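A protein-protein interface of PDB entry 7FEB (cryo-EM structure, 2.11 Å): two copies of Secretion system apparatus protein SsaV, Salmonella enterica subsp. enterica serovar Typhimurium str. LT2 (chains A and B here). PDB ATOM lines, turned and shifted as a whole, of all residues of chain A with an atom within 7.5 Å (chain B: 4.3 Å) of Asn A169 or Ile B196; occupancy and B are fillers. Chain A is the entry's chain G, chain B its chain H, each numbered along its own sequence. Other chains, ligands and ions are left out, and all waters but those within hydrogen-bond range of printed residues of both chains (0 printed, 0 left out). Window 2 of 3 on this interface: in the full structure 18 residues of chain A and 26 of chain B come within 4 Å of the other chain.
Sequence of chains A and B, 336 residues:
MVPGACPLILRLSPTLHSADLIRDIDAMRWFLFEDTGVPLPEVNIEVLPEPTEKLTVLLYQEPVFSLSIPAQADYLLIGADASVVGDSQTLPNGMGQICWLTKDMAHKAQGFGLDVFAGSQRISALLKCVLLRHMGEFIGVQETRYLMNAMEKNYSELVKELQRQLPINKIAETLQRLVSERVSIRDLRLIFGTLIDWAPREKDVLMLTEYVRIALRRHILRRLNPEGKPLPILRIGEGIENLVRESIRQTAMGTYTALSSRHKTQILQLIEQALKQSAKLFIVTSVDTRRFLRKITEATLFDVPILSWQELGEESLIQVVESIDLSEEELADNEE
OE1 of Gln A142 lies within hydrogen-bond range of N of Leu B158, at 3.3 Å.
NH2 of Arg B164 sits at hydrogen-bond distance from OD1 of Asn A169 (3.4 Å).
The side-chain carboxylate (OE2) of Glu B161 sits close to the side-chain amide oxygen (OD1) of Asn A169, 3.1 Å away.
OE1 of Glu B161 is in salt-bridge range of NE of Arg B164 (3.2 Å).
Among the printed residues, pairs that only touch across the chains: Val A141 with Leu B158 (3.96 Å), Pro A167 with Arg B164 (3.7 Å), Ile A168 with Glu B161 (3.6 Å) and Asn A169 with Ile B196 (3.9 Å).
Asn A169 touches just these residues of chain B: Glu B161, Arg B164 and Ile B196.
Ile B196 touches just one residue of chain A: Asn A169 (3.9 Å).
Of the printed residues of chain A, Glu B161 touches Ile A168 (3.6 Å) and Asn A169 (3.1 Å).
Of the printed residues of chain B, Gln A142 touches Leu B158 (3.3 Å).
Printed residues of chain B within 4 Å of Val A141: Leu B158 (3.96 Å).
Printed residues of chain B within 4 Å of Pro A167: Arg B164.
Of the printed residues of chain A, Arg B164 touches Pro A167 (3.7 Å) and Asn A169 (3.4 Å).
Leu B162 touches none of the printed residues of chain A.
Leu B195 touches none of the printed residues of chain A.
The nearest printed residue of chain B that does not touch Asn A169 is Pro B200 (5.1 Å).
The nearest printed residue of chain B that does not touch Gln A142 is Ile B196 (7.4 Å).
Hydrophobic or aromatic side chains of chain A within 4 Å of the printed part of chain B: Val A141, Pro A167 and Ile A168.
Hydrophobic or aromatic side chains of chain B within 4 Å of the printed part of chain A: Leu B158 and Ile B196.
Along chain B the printed residues that touch a printed residue of chain A span positions 158 to 196.
Among the printed residues, 7 pairs touch across the chains.
Among the printed residues, no Asp or Glu carboxylate lies within 4 Å of a Lys or Arg side-chain nitrogen of the other chain.
No position is printed for both chains.
Of the 7 pairs that touch across the chains among the printed residues, none has its exchanged pair printed and touching as well.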
ATOM      1  N   GLY A 140       5.497  23.936   7.950  1.00  0.00           N
ATOM      2  CA  GLY A 140       6.127  24.315   9.199  1.00  0.00           C
ATOM      3  C   GLY A 140       6.998  25.543   9.039  1.00  0.00           C
ATOM      4  O   GLY A 140       6.797  26.323   8.107  1.00  0.00           O
ATOM      5  N   VAL A 141       7.972  25.721   9.932  1.00  0.00           N
ATOM      6  CA  VAL A 141       8.815  26.914   9.894  1.00  0.00           C
ATOM      7  C   VAL A 141       9.647  26.947   8.617  1.00  0.00           C
ATOM      8  O   VAL A 141       9.750  27.983   7.950  1.00  0.00           O
ATOM      9  CB  VAL A 141       9.699  26.987  11.154  1.00  0.00           C
ATOM     10  CG1 VAL A 141      10.917  27.867  10.915  1.00  0.00           C
ATOM     11  CG2 VAL A 141       8.896  27.504  12.335  1.00  0.00           C
ATOM     12  N   GLN A 142      10.254  25.813   8.254  1.00  0.00           N
ATOM     13  CA  GLN A 142      11.078  25.766   7.049  1.00  0.00           C
ATOM     14  C   GLN A 142      10.242  25.975   5.790  1.00  0.00           C
ATOM     15  O   GLN A 142      10.661  26.683   4.868  1.00  0.00           O
ATOM     16  CB  GLN A 142      11.827  24.434   6.977  1.00  0.00           C
ATOM     17  CG  GLN A 142      12.816  24.344   5.832  1.00  0.00           C
ATOM     18  CD  GLN A 142      13.917  25.378   5.935  1.00  0.00           C
ATOM     19  OE1 GLN A 142      14.413  25.661   7.021  1.00  0.00           O
ATOM     20  NE2 GLN A 142      14.302  25.948   4.806  1.00  0.00           N
ATOM     21  N   THR A 144       7.335  27.549   5.626  1.00  0.00           N
ATOM     22  CA  THR A 144       6.930  28.948   5.645  1.00  0.00           C
ATOM     23  C   THR A 144       8.057  29.849   5.154  1.00  0.00           C
ATOM     24  O   THR A 144       7.817  30.806   4.408  1.00  0.00           O
ATOM     25  CB  THR A 144       6.498  29.344   7.056  1.00  0.00           C
ATOM     26  OG1 THR A 144       5.407  28.513   7.467  1.00  0.00           O
ATOM     27  CG2 THR A 144       6.069  30.797   7.107  1.00  0.00           C
ATOM     28  N   LEU A 166       5.744  40.322  12.464  1.00  0.00           N
ATOM     29  CA  LEU A 166       5.613  39.042  13.142  1.00  0.00           C
ATOM     30  C   LEU A 166       6.880  38.214  13.004  1.00  0.00           C
ATOM     31  O   LEU A 166       7.576  38.297  11.988  1.00  0.00           O
ATOM     32  CB  LEU A 166       4.429  38.241  12.579  1.00  0.00           C
ATOM     33  CG  LEU A 166       3.023  38.654  13.008  1.00  0.00           C
ATOM     34  CD1 LEU A 166       1.984  37.936  12.169  1.00  0.00           C
ATOM     35  CD2 LEU A 166       2.810  38.371  14.483  1.00  0.00           C
ATOM     36  N   PRO A 167       7.201  37.406  14.010  1.00  0.00           N
ATOM     37  CA  PRO A 167       8.285  36.431  13.864  1.00  0.00           C
ATOM     38  C   PRO A 167       7.821  35.212  13.079  1.00  0.00           C
ATOM     39  O   PRO A 167       6.630  34.921  12.974  1.00  0.00           O
ATOM     40  CB  PRO A 167       8.631  36.065  15.311  1.00  0.00           C
ATOM     41  CG  PRO A 167       7.370  36.287  16.061  1.00  0.00           C
ATOM     42  CD  PRO A 167       6.610  37.382  15.360  1.00  0.00           C
ATOM     43  N   ILE A 168       8.799  34.490  12.525  1.00  0.00           N
ATOM     44  CA  ILE A 168       8.485  33.429  11.570  1.00  0.00           C
ATOM     45  C   ILE A 168       7.697  32.298  12.224  1.00  0.00           C
ATOM     46  O   ILE A 168       6.899  31.631  11.559  1.00  0.00           O
ATOM     47  CB  ILE A 168       9.769  32.905  10.894  1.00  0.00           C
ATOM     48  CG1 ILE A 168       9.413  31.993   9.715  1.00  0.00           C
ATOM     49  CG2 ILE A 168      10.656  32.176  11.893  1.00  0.00           C
ATOM     50  CD1 ILE A 168      10.497  31.872   8.680  1.00  0.00           C
ATOM     51  N   ASN A 169       7.896  32.064  13.523  1.00  0.00           N
ATOM     52  CA  ASN A 169       7.164  30.987  14.182  1.00  0.00           C
ATOM     53  C   ASN A 169       5.665  31.267  14.203  1.00  0.00           C
ATOM     54  O   ASN A 169       4.857  30.360  13.979  1.00  0.00           O
ATOM     55  CB  ASN A 169       7.699  30.765  15.599  1.00  0.00           C
ATOM     56  CG  ASN A 169       8.003  32.059  16.325  1.00  0.00           C
ATOM     57  OD1 ASN A 169       8.875  32.824  15.916  1.00  0.00           O
ATOM     58  ND2 ASN A 169       7.290  32.306  17.414  1.00  0.00           N
ATOM     59  N   LYS A 170       5.275  32.519  14.449  1.00  0.00           N
ATOM     60  CA  LYS A 170       3.856  32.864  14.450  1.00  0.00           C
ATOM     61  C   LYS A 170       3.257  32.790  13.048  1.00  0.00           C
ATOM     62  O   LYS A 170       2.119  32.340  12.880  1.00  0.00           O
ATOM     63  CB  LYS A 170       3.656  34.254  15.050  1.00  0.00           C
ATOM     64  CG  LYS A 170       4.267  34.423  16.427  1.00  0.00           C
ATOM     65  CD  LYS A 170       3.318  35.149  17.359  1.00  0.00           C
ATOM     66  CE  LYS A 170       4.015  35.558  18.643  1.00  0.00           C
ATOM     67  NZ  LYS A 170       3.051  36.086  19.644  1.00  0.00           N
ATOM     68  N   ILE A 171       4.006  33.229  12.033  1.00  0.00           N
ATOM     69  CA  ILE A 171       3.532  33.121  10.654  1.00  0.00           C
ATOM     70  C   ILE A 171       3.331  31.660  10.275  1.00  0.00           C
ATOM     71  O   ILE A 171       2.321  31.290   9.659  1.00  0.00           O
ATOM     72  CB  ILE A 171       4.513  33.822   9.695  1.00  0.00           C
ATOM     73  CG1 ILE A 171       4.716  35.283  10.102  1.00  0.00           C
ATOM     74  CG2 ILE A 171       4.021  33.725   8.258  1.00  0.00           C
ATOM     75  CD1 ILE A 171       6.009  35.880   9.598  1.00  0.00           C
ATOM     76  N   ALA A 172       4.292  30.806  10.637  1.00  0.00           N
ATOM     77  CA  ALA A 172       4.176  29.381  10.356  1.00  0.00           C
ATOM     78  C   ALA A 172       2.993  28.770  11.090  1.00  0.00           C
ATOM     79  O   ALA A 172       2.276  27.935  10.534  1.00  0.00           O
ATOM     80  CB  ALA A 172       5.472  28.666  10.734  1.00  0.00           C
ATOM     81  N   GLU A 173       2.777  29.172  12.344  1.00  0.00           N
ATOM     82  CA  GLU A 173       1.633  28.665  13.095  1.00  0.00           C
ATOM     83  C   GLU A 173       0.317  29.067  12.438  1.00  0.00           C
ATOM     84  O   GLU A 173      -0.606  28.252  12.335  1.00  0.00           O
ATOM     85  CB  GLU A 173       1.692  29.168  14.535  1.00  0.00           C
ATOM     86  CG  GLU A 173       0.871  28.350  15.510  1.00  0.00           C
ATOM     87  CD  GLU A 173       0.826  28.971  16.890  1.00  0.00           C
ATOM     88  OE1 GLU A 173       1.828  29.598  17.293  1.00  0.00           O
ATOM     89  OE2 GLU A 173      -0.210  28.833  17.572  1.00  0.00           O
ATOM     90  N   THR A 174       0.215  30.318  11.984  1.00  0.00           N
ATOM     91  CA  THR A 174      -1.000  30.769  11.307  1.00  0.00           C
ATOM     92  C   THR A 174      -1.237  29.987  10.020  1.00  0.00           C
ATOM     93  O   THR A 174      -2.359  29.544   9.744  1.00  0.00           O
ATOM     94  CB  THR A 174      -0.915  32.269  11.018  1.00  0.00           C
ATOM     95  OG1 THR A 174      -0.729  32.986  12.243  1.00  0.00           O
ATOM     96  CG2 THR A 174      -2.183  32.757  10.338  1.00  0.00           C
ATOM     97  N   LEU A 175      -0.185  29.804   9.217  1.00  0.00           N
ATOM     98  CA  LEU A 175      -0.329  29.059   7.970  1.00  0.00           C
ATOM     99  C   LEU A 175      -0.726  27.611   8.231  1.00  0.00           C
ATOM    100  O   LEU A 175      -1.574  27.053   7.523  1.00  0.00           O
ATOM    101  CB  LEU A 175       0.969  29.121   7.166  1.00  0.00           C
ATOM    102  CG  LEU A 175       1.351  30.474   6.561  1.00  0.00           C
ATOM    103  CD1 LEU A 175       2.533  30.323   5.622  1.00  0.00           C
ATOM    104  CD2 LEU A 175       0.167  31.111   5.847  1.00  0.00           C
ATOM    105  N   VAL A 205      -2.244  34.121  17.991  1.00  0.00           N
ATOM    106  CA  VAL A 205      -2.165  33.510  16.668  1.00  0.00           C
ATOM    107  C   VAL A 205      -3.527  32.981  16.237  1.00  0.00           C
ATOM    108  O   VAL A 205      -3.880  33.033  15.053  1.00  0.00           O
ATOM    109  CB  VAL A 205      -1.085  32.412  16.658  1.00  0.00           C
ATOM    110  CG1 VAL A 205      -1.273  31.465  15.482  1.00  0.00           C
ATOM    111  CG2 VAL A 205       0.297  33.038  16.614  1.00  0.00           C
ATOM    112  N   LEU B 158      14.625  26.272  10.278  1.00  0.00           N
ATOM    113  CA  LEU B 158      14.106  25.587  11.457  1.00  0.00           C
ATOM    114  C   LEU B 158      15.156  25.507  12.561  1.00  0.00           C
ATOM    115  O   LEU B 158      14.857  25.764  13.733  1.00  0.00           O
ATOM    116  CB  LEU B 158      13.621  24.191  11.066  1.00  0.00           C
ATOM    117  CG  LEU B 158      13.006  23.297  12.142  1.00  0.00           C
ATOM    118  CD1 LEU B 158      11.653  23.824  12.565  1.00  0.00           C
ATOM    119  CD2 LEU B 158      12.892  21.870  11.642  1.00  0.00           C
ATOM    120  N   GLU B 161      15.683  28.992  14.066  1.00  0.00           N
ATOM    121  CA  GLU B 161      14.596  29.379  14.959  1.00  0.00           C
ATOM    122  C   GLU B 161      14.649  28.601  16.268  1.00  0.00           C
ATOM    123  O   GLU B 161      14.385  29.162  17.340  1.00  0.00           O
ATOM    124  CB  GLU B 161      13.250  29.181  14.260  1.00  0.00           C
ATOM    125  CG  GLU B 161      12.041  29.654  15.057  1.00  0.00           C
ATOM    126  CD  GLU B 161      12.128  31.112  15.476  1.00  0.00           C
ATOM    127  OE1 GLU B 161      12.770  31.912  14.763  1.00  0.00           O
ATOM    128  OE2 GLU B 161      11.548  31.460  16.523  1.00  0.00           O
ATOM    129  N   LEU B 162      14.985  27.312  16.201  1.00  0.00           N
ATOM    130  CA  LEU B 162      15.129  26.523  17.420  1.00  0.00           C
ATOM    131  C   LEU B 162      16.235  27.079  18.308  1.00  0.00           C
ATOM    132  O   LEU B 162      16.068  27.182  19.527  1.00  0.00           O
ATOM    133  CB  LEU B 162      15.404  25.063  17.066  1.00  0.00           C
ATOM    134  CG  LEU B 162      15.722  24.122  18.229  1.00  0.00           C
ATOM    135  CD1 LEU B 162      14.464  23.779  18.999  1.00  0.00           C
ATOM    136  CD2 LEU B 162      16.412  22.869  17.727  1.00  0.00           C
ATOM    137  N   ARG B 164      17.232  30.165  18.324  1.00  0.00           N
ATOM    138  CA  ARG B 164      16.675  31.405  18.852  1.00  0.00           C
ATOM    139  C   ARG B 164      15.773  31.150  20.053  1.00  0.00           C
ATOM    140  O   ARG B 164      15.719  31.973  20.973  1.00  0.00           O
ATOM    141  CB  ARG B 164      15.905  32.137  17.753  1.00  0.00           C
ATOM    142  CG  ARG B 164      15.394  33.509  18.138  1.00  0.00           C
ATOM    143  CD  ARG B 164      14.884  34.265  16.917  1.00  0.00           C
ATOM    144  NE  ARG B 164      13.429  34.236  16.796  1.00  0.00           N
ATOM    145  CZ  ARG B 164      12.573  34.721  17.687  1.00  0.00           C
ATOM    146  NH1 ARG B 164      12.985  35.346  18.779  1.00  0.00           N
ATOM    147  NH2 ARG B 164      11.267  34.588  17.470  1.00  0.00           N
ATOM    148  N   PHE B 192      11.791  19.443  16.521  1.00  0.00           N
ATOM    149  CA  PHE B 192      12.211  20.841  16.536  1.00  0.00           C
ATOM    150  C   PHE B 192      11.018  21.775  16.401  1.00  0.00           C
ATOM    151  O   PHE B 192      10.967  22.822  17.056  1.00  0.00           O
ATOM    152  CB  PHE B 192      13.228  21.102  15.425  1.00  0.00           C
ATOM    153  CG  PHE B 192      14.560  20.438  15.643  1.00  0.00           C
ATOM    154  CD1 PHE B 192      14.856  19.814  16.843  1.00  0.00           C
ATOM    155  CD2 PHE B 192      15.515  20.438  14.644  1.00  0.00           C
ATOM    156  CE1 PHE B 192      16.076  19.205  17.039  1.00  0.00           C
ATOM    157  CE2 PHE B 192      16.737  19.829  14.836  1.00  0.00           C
ATOM    158  CZ  PHE B 192      17.017  19.212  16.035  1.00  0.00           C
ATOM    159  N   GLY B 193      10.046  21.417  15.557  1.00  0.00           N
ATOM    160  CA  GLY B 193       8.847  22.229  15.446  1.00  0.00           C
ATOM    161  C   GLY B 193       8.070  22.305  16.746  1.00  0.00           C
ATOM    162  O   GLY B 193       7.607  23.377  17.140  1.00  0.00           O
ATOM    163  N   THR B 194       7.922  21.169  17.432  1.00  0.00           N
ATOM    164  CA  THR B 194       7.235  21.161  18.720  1.00  0.00           C
ATOM    165  C   THR B 194       7.980  21.998  19.751  1.00  0.00           C
ATOM    166  O   THR B 194       7.364  22.741  20.527  1.00  0.00           O
ATOM    167  CB  THR B 194       7.071  19.724  19.215  1.00  0.00           C
ATOM    168  OG1 THR B 194       6.497  18.924  18.176  1.00  0.00           O
ATOM    169  CG2 THR B 194       6.176  19.677  20.439  1.00  0.00           C
ATOM    170  N   LEU B 195       9.310  21.890  19.774  1.00  0.00           N
ATOM    171  CA  LEU B 195      10.096  22.681  20.715  1.00  0.00           C
ATOM    172  C   LEU B 195       9.966  24.169  20.424  1.00  0.00           C
ATOM    173  O   LEU B 195       9.900  24.984  21.351  1.00  0.00           O
ATOM    174  CB  LEU B 195      11.562  22.250  20.672  1.00  0.00           C
ATOM    175  CG  LEU B 195      11.887  20.902  21.315  1.00  0.00           C
ATOM    176  CD1 LEU B 195      13.331  20.523  21.050  1.00  0.00           C
ATOM    177  CD2 LEU B 195      11.601  20.936  22.805  1.00  0.00           C
ATOM    178  N   ILE B 196       9.936  24.546  19.146  1.00  0.00           N
ATOM    179  CA  ILE B 196       9.734  25.946  18.787  1.00  0.00           C
ATOM    180  C   ILE B 196       8.352  26.414  19.224  1.00  0.00           C
ATOM    181  O   ILE B 196       8.192  27.522  19.748  1.00  0.00           O
ATOM    182  CB  ILE B 196       9.955  26.146  17.277  1.00  0.00           C
ATOM    183  CG1 ILE B 196      11.444  26.067  16.943  1.00  0.00           C
ATOM    184  CG2 ILE B 196       9.372  27.475  16.814  1.00  0.00           C
ATOM    185  CD1 ILE B 196      11.726  25.915  15.474  1.00  0.00           C
ATOM    186  N   ASP B 197       7.335  25.573  19.026  1.00  0.00           N
ATOM    187  CA  ASP B 197       5.977  25.949  19.402  1.00  0.00           C
ATOM    188  C   ASP B 197       5.852  26.171  20.904  1.00  0.00           C
ATOM    189  O   ASP B 197       5.214  27.134  21.343  1.00  0.00           O
ATOM    190  CB  ASP B 197       4.988  24.878  18.945  1.00  0.00           C
ATOM    191  CG  ASP B 197       4.664  24.979  17.472  1.00  0.00           C
ATOM    192  OD1 ASP B 197       4.866  26.064  16.890  1.00  0.00           O
ATOM    193  OD2 ASP B 197       4.205  23.971  16.893  1.00  0.00           O
ATOM    194  N   TRP B 198       6.453  25.296  21.709  1.00  0.00           N
ATOM    195  CA  TRP B 198       6.204  25.316  23.146  1.00  0.00           C
ATOM    196  C   TRP B 198       7.269  26.044  23.959  1.00  0.00           C
ATOM    197  O   TRP B 198       7.043  26.294  25.146  1.00  0.00           O
ATOM    198  CB  TRP B 198       6.055  23.887  23.672  1.00  0.00           C
ATOM    199  CG  TRP B 198       4.737  23.281  23.340  1.00  0.00           C
ATOM    200  CD1 TRP B 198       4.478  22.364  22.368  1.00  0.00           C
ATOM    201  CD2 TRP B 198       3.485  23.560  23.973  1.00  0.00           C
ATOM    202  NE1 TRP B 198       3.145  22.046  22.360  1.00  0.00           N
ATOM    203  CE2 TRP B 198       2.512  22.767  23.337  1.00  0.00           C
ATOM    204  CE3 TRP B 198       3.093  24.400  25.020  1.00  0.00           C
ATOM    205  CZ2 TRP B 198       1.171  22.790  23.711  1.00  0.00           C
ATOM    206  CZ3 TRP B 198       1.764  24.420  25.389  1.00  0.00           C
ATOM    207  CH2 TRP B 198       0.819  23.621  24.736  1.00  0.00           C
ATOM    208  N   ALA B 199       8.409  26.387  23.366  1.00  0.00           N
ATOM    209  CA  ALA B 199       9.469  27.051  24.123  1.00  0.00           C
ATOM    210  C   ALA B 199       9.052  28.396  24.706  1.00  0.00           C
ATOM    211  O   ALA B 199       9.375  28.658  25.878  1.00  0.00           O
ATOM    212  CB  ALA B 199      10.721  27.186  23.250  1.00  0.00           C
ATOM    213  N   PRO B 200       8.381  29.296  23.975  1.00  0.00           N
ATOM    214  CA  PRO B 200       7.975  30.566  24.604  1.00  0.00           C
ATOM    215  C   PRO B 200       7.041  30.394  25.788  1.00  0.00           C
ATOM    216  O   PRO B 200       7.082  31.209  26.718  1.00  0.00           O
ATOM    217  CB  PRO B 200       7.295  31.324  23.455  1.00  0.00           C
ATOM    218  CG  PRO B 200       7.861  30.731  22.224  1.00  0.00           C
ATOM    219  CD  PRO B 200       8.052  29.285  22.538  1.00  0.00           C
